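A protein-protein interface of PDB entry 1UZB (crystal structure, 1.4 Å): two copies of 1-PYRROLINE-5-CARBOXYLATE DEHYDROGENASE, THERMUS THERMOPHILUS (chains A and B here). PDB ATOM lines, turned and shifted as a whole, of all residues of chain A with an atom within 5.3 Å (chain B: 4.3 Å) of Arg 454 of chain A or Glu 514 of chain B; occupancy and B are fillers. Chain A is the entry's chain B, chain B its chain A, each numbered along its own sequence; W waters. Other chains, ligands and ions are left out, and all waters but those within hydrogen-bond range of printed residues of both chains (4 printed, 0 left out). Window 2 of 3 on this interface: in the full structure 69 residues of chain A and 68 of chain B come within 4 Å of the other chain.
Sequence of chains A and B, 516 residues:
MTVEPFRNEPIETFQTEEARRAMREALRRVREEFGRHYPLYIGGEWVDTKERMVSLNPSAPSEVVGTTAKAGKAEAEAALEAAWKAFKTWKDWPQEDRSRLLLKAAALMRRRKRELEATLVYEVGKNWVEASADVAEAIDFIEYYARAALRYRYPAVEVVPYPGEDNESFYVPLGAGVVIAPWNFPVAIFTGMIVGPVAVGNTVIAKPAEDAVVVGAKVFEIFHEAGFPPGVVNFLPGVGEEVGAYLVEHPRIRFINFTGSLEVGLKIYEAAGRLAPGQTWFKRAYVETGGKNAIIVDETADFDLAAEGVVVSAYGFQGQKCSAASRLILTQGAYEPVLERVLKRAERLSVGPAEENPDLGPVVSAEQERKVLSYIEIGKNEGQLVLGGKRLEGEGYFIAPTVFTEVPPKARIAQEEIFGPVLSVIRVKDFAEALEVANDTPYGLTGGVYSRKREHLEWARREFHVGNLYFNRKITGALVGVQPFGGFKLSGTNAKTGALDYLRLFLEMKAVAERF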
ATOM      1  N   ARG A 452      -9.937 -32.736  17.082  1.00  0.00           N
ATOM      2  CA  ARG A 452      -8.510 -32.523  16.870  1.00  0.00           C
ATOM      3  C   ARG A 452      -8.269 -31.040  16.592  1.00  0.00           C
ATOM      4  O   ARG A 452      -7.127 -30.579  16.598  1.00  0.00           O
ATOM      5  CB  ARG A 452      -7.996 -33.322  15.670  1.00  0.00           C
ATOM      6  CG  ARG A 452      -7.872 -34.823  15.859  1.00  0.00           C
ATOM      7  CD  ARG A 452      -7.051 -35.384  14.702  1.00  0.00           C
ATOM      8  NE  ARG A 452      -6.796 -36.819  14.794  1.00  0.00           N
ATOM      9  CZ  ARG A 452      -7.645 -37.764  14.401  1.00  0.00           C
ATOM     10  NH1 ARG A 452      -7.316 -39.043  14.527  1.00  0.00           N
ATOM     11  NH2 ARG A 452      -8.816 -37.435  13.872  1.00  0.00           N
ATOM     12  N   LYS A 453      -9.341 -30.290  16.348  1.00  0.00           N
ATOM     13  CA  LYS A 453      -9.206 -28.871  16.040  1.00  0.00           C
ATOM     14  C   LYS A 453      -8.946 -28.042  17.292  1.00  0.00           C
ATOM     15  O   LYS A 453      -9.822 -27.893  18.147  1.00  0.00           O
ATOM     16  CB  LYS A 453     -10.457 -28.368  15.315  1.00  0.00           C
ATOM     17  CG  LYS A 453     -10.339 -26.938  14.806  1.00  0.00           C
ATOM     18  CD  LYS A 453     -11.459 -26.598  13.838  1.00  0.00           C
ATOM     19  CE  LYS A 453     -11.366 -25.153  13.373  1.00  0.00           C
ATOM     20  NZ  LYS A 453     -10.046 -24.857  12.754  1.00  0.00           N
ATOM     21  N   ARG A 454      -7.734 -27.505  17.392  1.00  0.00           N
ATOM     22  CA  ARG A 454      -7.334 -26.709  18.546  1.00  0.00           C
ATOM     23  C   ARG A 454      -8.299 -25.574  18.858  1.00  0.00           C
ATOM     24  O   ARG A 454      -8.623 -25.324  20.021  1.00  0.00           O
ATOM     25  CB  ARG A 454      -5.932 -26.120  18.335  1.00  0.00           C
ATOM     26  CG  ARG A 454      -4.851 -27.124  17.957  1.00  0.00           C
ATOM     27  CD  ARG A 454      -4.826 -28.324  18.893  1.00  0.00           C
ATOM     28  NE  ARG A 454      -4.702 -27.957  20.303  1.00  0.00           N
ATOM     29  CZ  ARG A 454      -4.759 -28.835  21.300  1.00  0.00           C
ATOM     30  NH1 ARG A 454      -4.642 -28.428  22.555  1.00  0.00           N
ATOM     31  NH2 ARG A 454      -4.930 -30.123  21.042  1.00  0.00           N
ATOM     32  N   GLU A 455      -8.757 -24.883  17.818  1.00  0.00           N
ATOM     33  CA  GLU A 455      -9.660 -23.759  17.996  1.00  0.00           C
ATOM     34  C   GLU A 455     -10.996 -24.166  18.610  1.00  0.00           C
ATOM     35  O   GLU A 455     -11.622 -23.382  19.325  1.00  0.00           O
ATOM     36  CB  GLU A 455      -9.876 -23.042  16.661  1.00  0.00           C
ATOM     37  CG  GLU A 455      -8.611 -22.375  16.105  1.00  0.00           C
ATOM     38  CD  GLU A 455      -7.722 -23.318  15.297  1.00  0.00           C
ATOM     39  OE1 GLU A 455      -7.955 -24.545  15.307  1.00  0.00           O
ATOM     40  OE2 GLU A 455      -6.777 -22.819  14.650  1.00  0.00           O
ATOM     41  N   HIS A 456     -11.434 -25.389  18.337  1.00  0.00           N
ATOM     42  CA  HIS A 456     -12.688 -25.866  18.902  1.00  0.00           C
ATOM     43  C   HIS A 456     -12.494 -26.212  20.377  1.00  0.00           C
ATOM     44  O   HIS A 456     -13.339 -25.893  21.210  1.00  0.00           O
ATOM     45  CB  HIS A 456     -13.197 -27.085  18.130  1.00  0.00           C
ATOM     46  CG  HIS A 456     -13.785 -26.749  16.794  1.00  0.00           C
ATOM     47  ND1 HIS A 456     -14.365 -27.695  15.977  1.00  0.00           N
ATOM     48  CD2 HIS A 456     -13.905 -25.566  16.145  1.00  0.00           C
ATOM     49  CE1 HIS A 456     -14.819 -27.109  14.883  1.00  0.00           C
ATOM     50  NE2 HIS A 456     -14.553 -25.818  14.960  1.00  0.00           N
ATOM     51  N   LEU A 457     -11.371 -26.848  20.699  1.00  0.00           N
ATOM     52  CA  LEU A 457     -11.084 -27.212  22.078  1.00  0.00           C
ATOM     53  C   LEU A 457     -10.934 -25.964  22.942  1.00  0.00           C
ATOM     54  O   LEU A 457     -11.541 -25.869  24.008  1.00  0.00           O
ATOM     55  CB  LEU A 457      -9.802 -28.049  22.158  1.00  0.00           C
ATOM     56  CG  LEU A 457      -9.825 -29.417  21.466  1.00  0.00           C
ATOM     57  CD1 LEU A 457      -8.476 -30.100  21.647  1.00  0.00           C
ATOM     58  CD2 LEU A 457     -10.945 -30.279  22.040  1.00  0.00           C
ATOM     59  N   GLU A 458     -10.138 -25.003  22.485  1.00  0.00           N
ATOM     60  CA  GLU A 458      -9.934 -23.792  23.269  1.00  0.00           C
ATOM     61  C   GLU A 458     -11.221 -22.971  23.374  1.00  0.00           C
ATOM     62  O   GLU A 458     -11.463 -22.301  24.378  1.00  0.00           O
ATOM     63  CB  GLU A 458      -8.778 -22.973  22.682  1.00  0.00           C
ATOM     64  CG  GLU A 458      -7.442 -23.745  22.652  1.00  0.00           C
ATOM     65  CD  GLU A 458      -7.003 -24.278  24.018  1.00  0.00           C
ATOM     66  OE1 GLU A 458      -6.003 -25.033  24.072  1.00  0.00           O
ATOM     67  OE2 GLU A 458      -7.647 -23.949  25.035  1.00  0.00           O
ATOM     68  N   TRP A 459     -12.053 -23.045  22.340  1.00  0.00           N
ATOM     69  CA  TRP A 459     -13.340 -22.355  22.320  1.00  0.00           C
ATOM     70  C   TRP A 459     -14.197 -22.968  23.438  1.00  0.00           C
ATOM     71  O   TRP A 459     -14.833 -22.257  24.219  1.00  0.00           O
ATOM     72  CB  TRP A 459     -13.990 -22.580  20.954  1.00  0.00           C
ATOM     73  CG  TRP A 459     -15.310 -21.915  20.711  1.00  0.00           C
ATOM     74  CD1 TRP A 459     -16.029 -21.149  21.581  1.00  0.00           C
ATOM     75  CD2 TRP A 459     -16.074 -21.976  19.501  1.00  0.00           C
ATOM     76  NE1 TRP A 459     -17.198 -20.730  20.987  1.00  0.00           N
ATOM     77  CE2 TRP A 459     -17.250 -21.223  19.709  1.00  0.00           C
ATOM     78  CE3 TRP A 459     -15.878 -22.595  18.258  1.00  0.00           C
ATOM     79  CZ2 TRP A 459     -18.229 -21.072  18.720  1.00  0.00           C
ATOM     80  CZ3 TRP A 459     -16.853 -22.446  17.274  1.00  0.00           C
ATOM     81  CH2 TRP A 459     -18.012 -21.690  17.514  1.00  0.00           C
ATOM     82  N   ARG A 461     -13.095 -24.546  26.042  1.00  0.00           N
ATOM     83  CA  ARG A 461     -12.474 -24.242  27.325  1.00  0.00           C
ATOM     84  C   ARG A 461     -13.068 -22.953  27.873  1.00  0.00           C
ATOM     85  O   ARG A 461     -13.258 -22.809  29.078  1.00  0.00           O
ATOM     86  CB  ARG A 461     -10.956 -24.083  27.162  1.00  0.00           C
ATOM     87  CG  ARG A 461     -10.205 -23.775  28.463  1.00  0.00           C
ATOM     88  CD  ARG A 461      -8.695 -23.695  28.224  1.00  0.00           C
ATOM     89  NE  ARG A 461      -8.175 -24.944  27.674  1.00  0.00           N
ATOM     90  CZ  ARG A 461      -7.725 -25.962  28.404  1.00  0.00           C
ATOM     91  NH1 ARG A 461      -7.709 -25.886  29.730  1.00  0.00           N
ATOM     92  NH2 ARG A 461      -7.324 -27.076  27.807  1.00  0.00           N
ATOM     93  N   PHE A 471     -11.290 -33.114  27.428  1.00  0.00           N
ATOM     94  CA  PHE A 471     -11.047 -33.188  25.993  1.00  0.00           C
ATOM     95  C   PHE A 471     -10.389 -34.500  25.583  1.00  0.00           C
ATOM     96  O   PHE A 471      -9.349 -34.884  26.122  1.00  0.00           O
ATOM     97  CB  PHE A 471     -10.158 -32.027  25.531  1.00  0.00           C
ATOM     98  CG  PHE A 471     -10.746 -30.667  25.779  1.00  0.00           C
ATOM     99  CD1 PHE A 471     -12.125 -30.473  25.791  1.00  0.00           C
ATOM    100  CD2 PHE A 471      -9.914 -29.568  25.967  1.00  0.00           C
ATOM    101  CE1 PHE A 471     -12.664 -29.199  25.988  1.00  0.00           C
ATOM    102  CE2 PHE A 471     -10.443 -28.293  26.163  1.00  0.00           C
ATOM    103  CZ  PHE A 471     -11.824 -28.109  26.174  1.00  0.00           C
ATOM    104  N   ASN A 472     -11.016 -35.179  24.624  1.00  0.00           N
ATOM    105  CA  ASN A 472     -10.527 -36.436  24.079  1.00  0.00           C
ATOM    106  C   ASN A 472     -10.301 -37.547  25.094  1.00  0.00           C
ATOM    107  O   ASN A 472      -9.331 -38.300  25.012  1.00  0.00           O
ATOM    108  CB  ASN A 472      -9.271 -36.172  23.243  1.00  0.00           C
ATOM    109  CG  ASN A 472      -9.578 -35.330  22.018  1.00  0.00           C
ATOM    110  OD1 ASN A 472     -10.581 -35.565  21.339  1.00  0.00           O
ATOM    111  ND2 ASN A 472      -8.731 -34.351  21.729  1.00  0.00           N
ATOM    112  N   GLY B 164       0.276 -37.863  30.865  1.00  0.00           N
ATOM    113  CA  GLY B 164      -0.320 -37.685  29.547  1.00  0.00           C
ATOM    114  C   GLY B 164      -1.481 -36.719  29.425  1.00  0.00           C
ATOM    115  O   GLY B 164      -2.198 -36.736  28.419  1.00  0.00           O
ATOM    116  N   GLU B 165      -1.652 -35.867  30.427  1.00  0.00           N
ATOM    117  CA  GLU B 165      -2.748 -34.908  30.445  1.00  0.00           C
ATOM    118  C   GLU B 165      -2.361 -33.534  30.947  1.00  0.00           C
ATOM    119  O   GLU B 165      -1.422 -33.377  31.730  1.00  0.00           O
ATOM    120  CB  GLU B 165      -3.855 -35.381  31.384  1.00  0.00           C
ATOM    121  CG  GLU B 165      -4.727 -36.511  30.926  1.00  0.00           C
ATOM    122  CD  GLU B 165      -5.848 -36.784  31.920  1.00  0.00           C
ATOM    123  OE1 GLU B 165      -6.726 -37.611  31.606  1.00  0.00           O
ATOM    124  OE2 GLU B 165      -5.850 -36.174  33.018  1.00  0.00           O
ATOM    125  N   ASP B 166      -3.114 -32.541  30.496  1.00  0.00           N
ATOM    126  CA  ASP B 166      -2.949 -31.186  30.988  1.00  0.00           C
ATOM    127  C   ASP B 166      -4.211 -30.990  31.827  1.00  0.00           C
ATOM    128  O   ASP B 166      -5.323 -31.227  31.352  1.00  0.00           O
ATOM    129  CB  ASP B 166      -2.922 -30.165  29.849  1.00  0.00           C
ATOM    130  CG  ASP B 166      -2.735 -28.743  30.352  1.00  0.00           C
ATOM    131  OD1 ASP B 166      -3.695 -27.942  30.290  1.00  0.00           O
ATOM    132  OD2 ASP B 166      -1.621 -28.428  30.817  1.00  0.00           O
ATOM    133  N   ALA B 513      -9.505 -30.669  31.556  1.00  0.00           N
ATOM    134  CA  ALA B 513      -8.469 -31.660  31.313  1.00  0.00           C
ATOM    135  C   ALA B 513      -8.392 -32.030  29.840  1.00  0.00           C
ATOM    136  O   ALA B 513      -9.423 -32.202  29.183  1.00  0.00           O
ATOM    137  CB  ALA B 513      -8.759 -32.916  32.131  1.00  0.00           C
ATOM    138  N   GLU B 514      -7.176 -32.125  29.312  1.00  0.00           N
ATOM    139  CA  GLU B 514      -6.998 -32.557  27.934  1.00  0.00           C
ATOM    140  C   GLU B 514      -6.049 -33.739  27.926  1.00  0.00           C
ATOM    141  O   GLU B 514      -4.921 -33.645  28.417  1.00  0.00           O
ATOM    142  CB  GLU B 514      -6.415 -31.473  27.013  1.00  0.00           C
ATOM    143  CG  GLU B 514      -6.252 -32.030  25.588  1.00  0.00           C
ATOM    144  CD  GLU B 514      -5.700 -31.058  24.562  1.00  0.00           C
ATOM    145  OE1 GLU B 514      -5.619 -29.846  24.840  1.00  0.00           O
ATOM    146  OE2 GLU B 514      -5.353 -31.526  23.452  1.00  0.00           O
ATOM    147  N   ARG B 515      -6.519 -34.861  27.393  1.00  0.00           N
ATOM    148  CA  ARG B 515      -5.685 -36.048  27.276  1.00  0.00           C
ATOM    149  C   ARG B 515      -5.065 -35.951  25.887  1.00  0.00           C
ATOM    150  O   ARG B 515      -5.775 -35.950  24.879  1.00  0.00           O
ATOM    151  CB  ARG B 515      -6.527 -37.317  27.394  1.00  0.00           C
ATOM    152  CG  ARG B 515      -5.699 -38.588  27.326  1.00  0.00           C
ATOM    153  CD  ARG B 515      -6.515 -39.798  27.726  1.00  0.00           C
ATOM    154  NE  ARG B 515      -6.968 -39.708  29.111  1.00  0.00           N
ATOM    155  CZ  ARG B 515      -7.648 -40.664  29.735  1.00  0.00           C
ATOM    156  NH1 ARG B 515      -8.022 -40.500  30.996  1.00  0.00           N
ATOM    157  NH2 ARG B 515      -7.950 -41.786  29.097  1.00  0.00           N
ATOM    158  N   PHE B 516      -3.744 -35.856  25.834  1.00  0.00           N
ATOM    159  CA  PHE B 516      -3.049 -35.719  24.558  1.00  0.00           C
ATOM    160  C   PHE B 516      -2.944 -36.999  23.740  1.00  0.00           C
ATOM    161  O   PHE B 516      -2.879 -36.884  22.497  1.00  0.00           O
ATOM    162  CB  PHE B 516      -1.661 -35.124  24.787  1.00  0.00           C
ATOM    163  CG  PHE B 516      -1.695 -33.772  25.430  1.00  0.00           C
ATOM    164  CD1 PHE B 516      -1.180 -33.583  26.707  1.00  0.00           C
ATOM    165  CD2 PHE B 516      -2.273 -32.692  24.770  1.00  0.00           C
ATOM    166  CE1 PHE B 516      -1.242 -32.336  27.319  1.00  0.00           C
ATOM    167  CE2 PHE B 516      -2.340 -31.442  25.373  1.00  0.00           C
ATOM    168  CZ  PHE B 516      -1.824 -31.266  26.652  1.00  0.00           C
ATOM    169  OXT PHE B 516      -2.910 -38.090  24.342  1.00  0.00           O
HETATM  170  O   HOH W   1      -7.221 -27.606  24.963  1.00  0.00           O
HETATM  171  O   HOH W   2      -6.142 -34.101  22.949  1.00  0.00           O
HETATM  172  O   HOH W   3      -6.825 -38.387  24.038  1.00  0.00           O
HETATM  173  O   HOH W   4      -6.350 -28.434  30.084  1.00  0.00           O
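N of Phe 471 of chain A is in hydrogen-bond range of O of Ala 513 of chain B, 2.7 Å away. The backbone carbonyl oxygen of Phe 471 of chain A is in hydrogen-bond range of the backbone NH of Arg 515 of chain B (3.1 Å). The side-chain carboxylate (OE2) of Glu 514 of chain B lies within salt-bridge range of the guanidinium group (NH2) of Arg 454 of chain A (2.8 Å).
OE1 of Glu 458 of chain A lies within salt-bridge range of NH1 of Arg 454 of chain A (3.96 Å). The side-chain carboxylate (OE1) of Glu 165 of chain B is in salt-bridge range of the guanidinium group (NH1) of Arg 515 of chain B, 3.2 Å away. The backbone carbonyl oxygen (O) of Asp 166 of chain B lies within hydrogen-bond range of the backbone NH (N) of Glu 514 of chain B (2.9 Å).
Among the printed residues, merely in contact across the chains: Leu 457 of chain A with Glu 514 of chain B, Phe 471 of chain A with Glu 514 of chain B and Asn 472 of chain A with Arg 515 of chain B.
Of chain B, only Glu 514 comes within 4 Å of Arg 454 of chain A. Of the printed residues of chain B, Leu 457 of chain A touches Glu 514 (3.9 Å). Arg 461 of chain A touches none of the printed residues of chain B. Of the printed residues of chain B, Phe 471 of chain A touches Ala 513, Glu 514 and Arg 515. Of the printed residues of chain B, Asn 472 of chain A touches Arg 515 (3.8 Å). Of the printed residues of chain A, Ala 513 of chain B touches Phe 471 (2.7 Å). Of chain A, only Arg 454, Leu 457 and Phe 471 come within 4 Å of Glu 514 of chain B. The nearest printed residue of chain B that does not touch Arg 454 of chain A is Phe 516 of chain B (4.7 Å).
Of the 11 printed residues of chain A, 4 touch a printed residue of chain B. Printed residues of chain A that touch a printed residue of chain B: Arg 454, Leu 457, Phe 471 and Asn 472. Along chain A the printed residues that touch a printed residue of chain B span positions 454 to 472. Of the 7 printed residues of chain B, 3 touch a printed residue of chain A. Among the printed residues, 6 pairs touch across the chains. Among the printed residues, Asp or Glu carboxylates within 4 Å of a Lys or Arg side-chain nitrogen of the other chain: Arg 454 of chain A with Glu 514 of chain B (2.8 Å).
No position is printed for both chains. Of the 6 pairs that touch across the chains among the printed residues, none has its exchanged pair printed and touching as well.
Water W3 lies within hydrogen-bond range of the backbone carbonyl oxygen (O) of Asn 472 of chain A (2.7 Å) and the backbone carbonyl oxygen (O) of Arg 515 of chain B (2.8 Å). Water W2 lies within hydrogen-bond range of O of Arg 515 of chain B, OE2 of Glu 514 of chain B and ND2 of Asn 472 of chain A. Water W4 lies within hydrogen-bond range of the side-chain carboxylate (OD1) of Asp 166 of chain B (2.7 Å) and the guanidinium group (NH2) of Arg 461 of chain A (2.8 Å). Water W1 lies within hydrogen-bond range of OE1 of Glu 514 of chain B (2.8 Å), NH2 of Arg 461 of chain A (2.9 Å) and OE1 of Glu 458 of chain A (3.0 Å).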
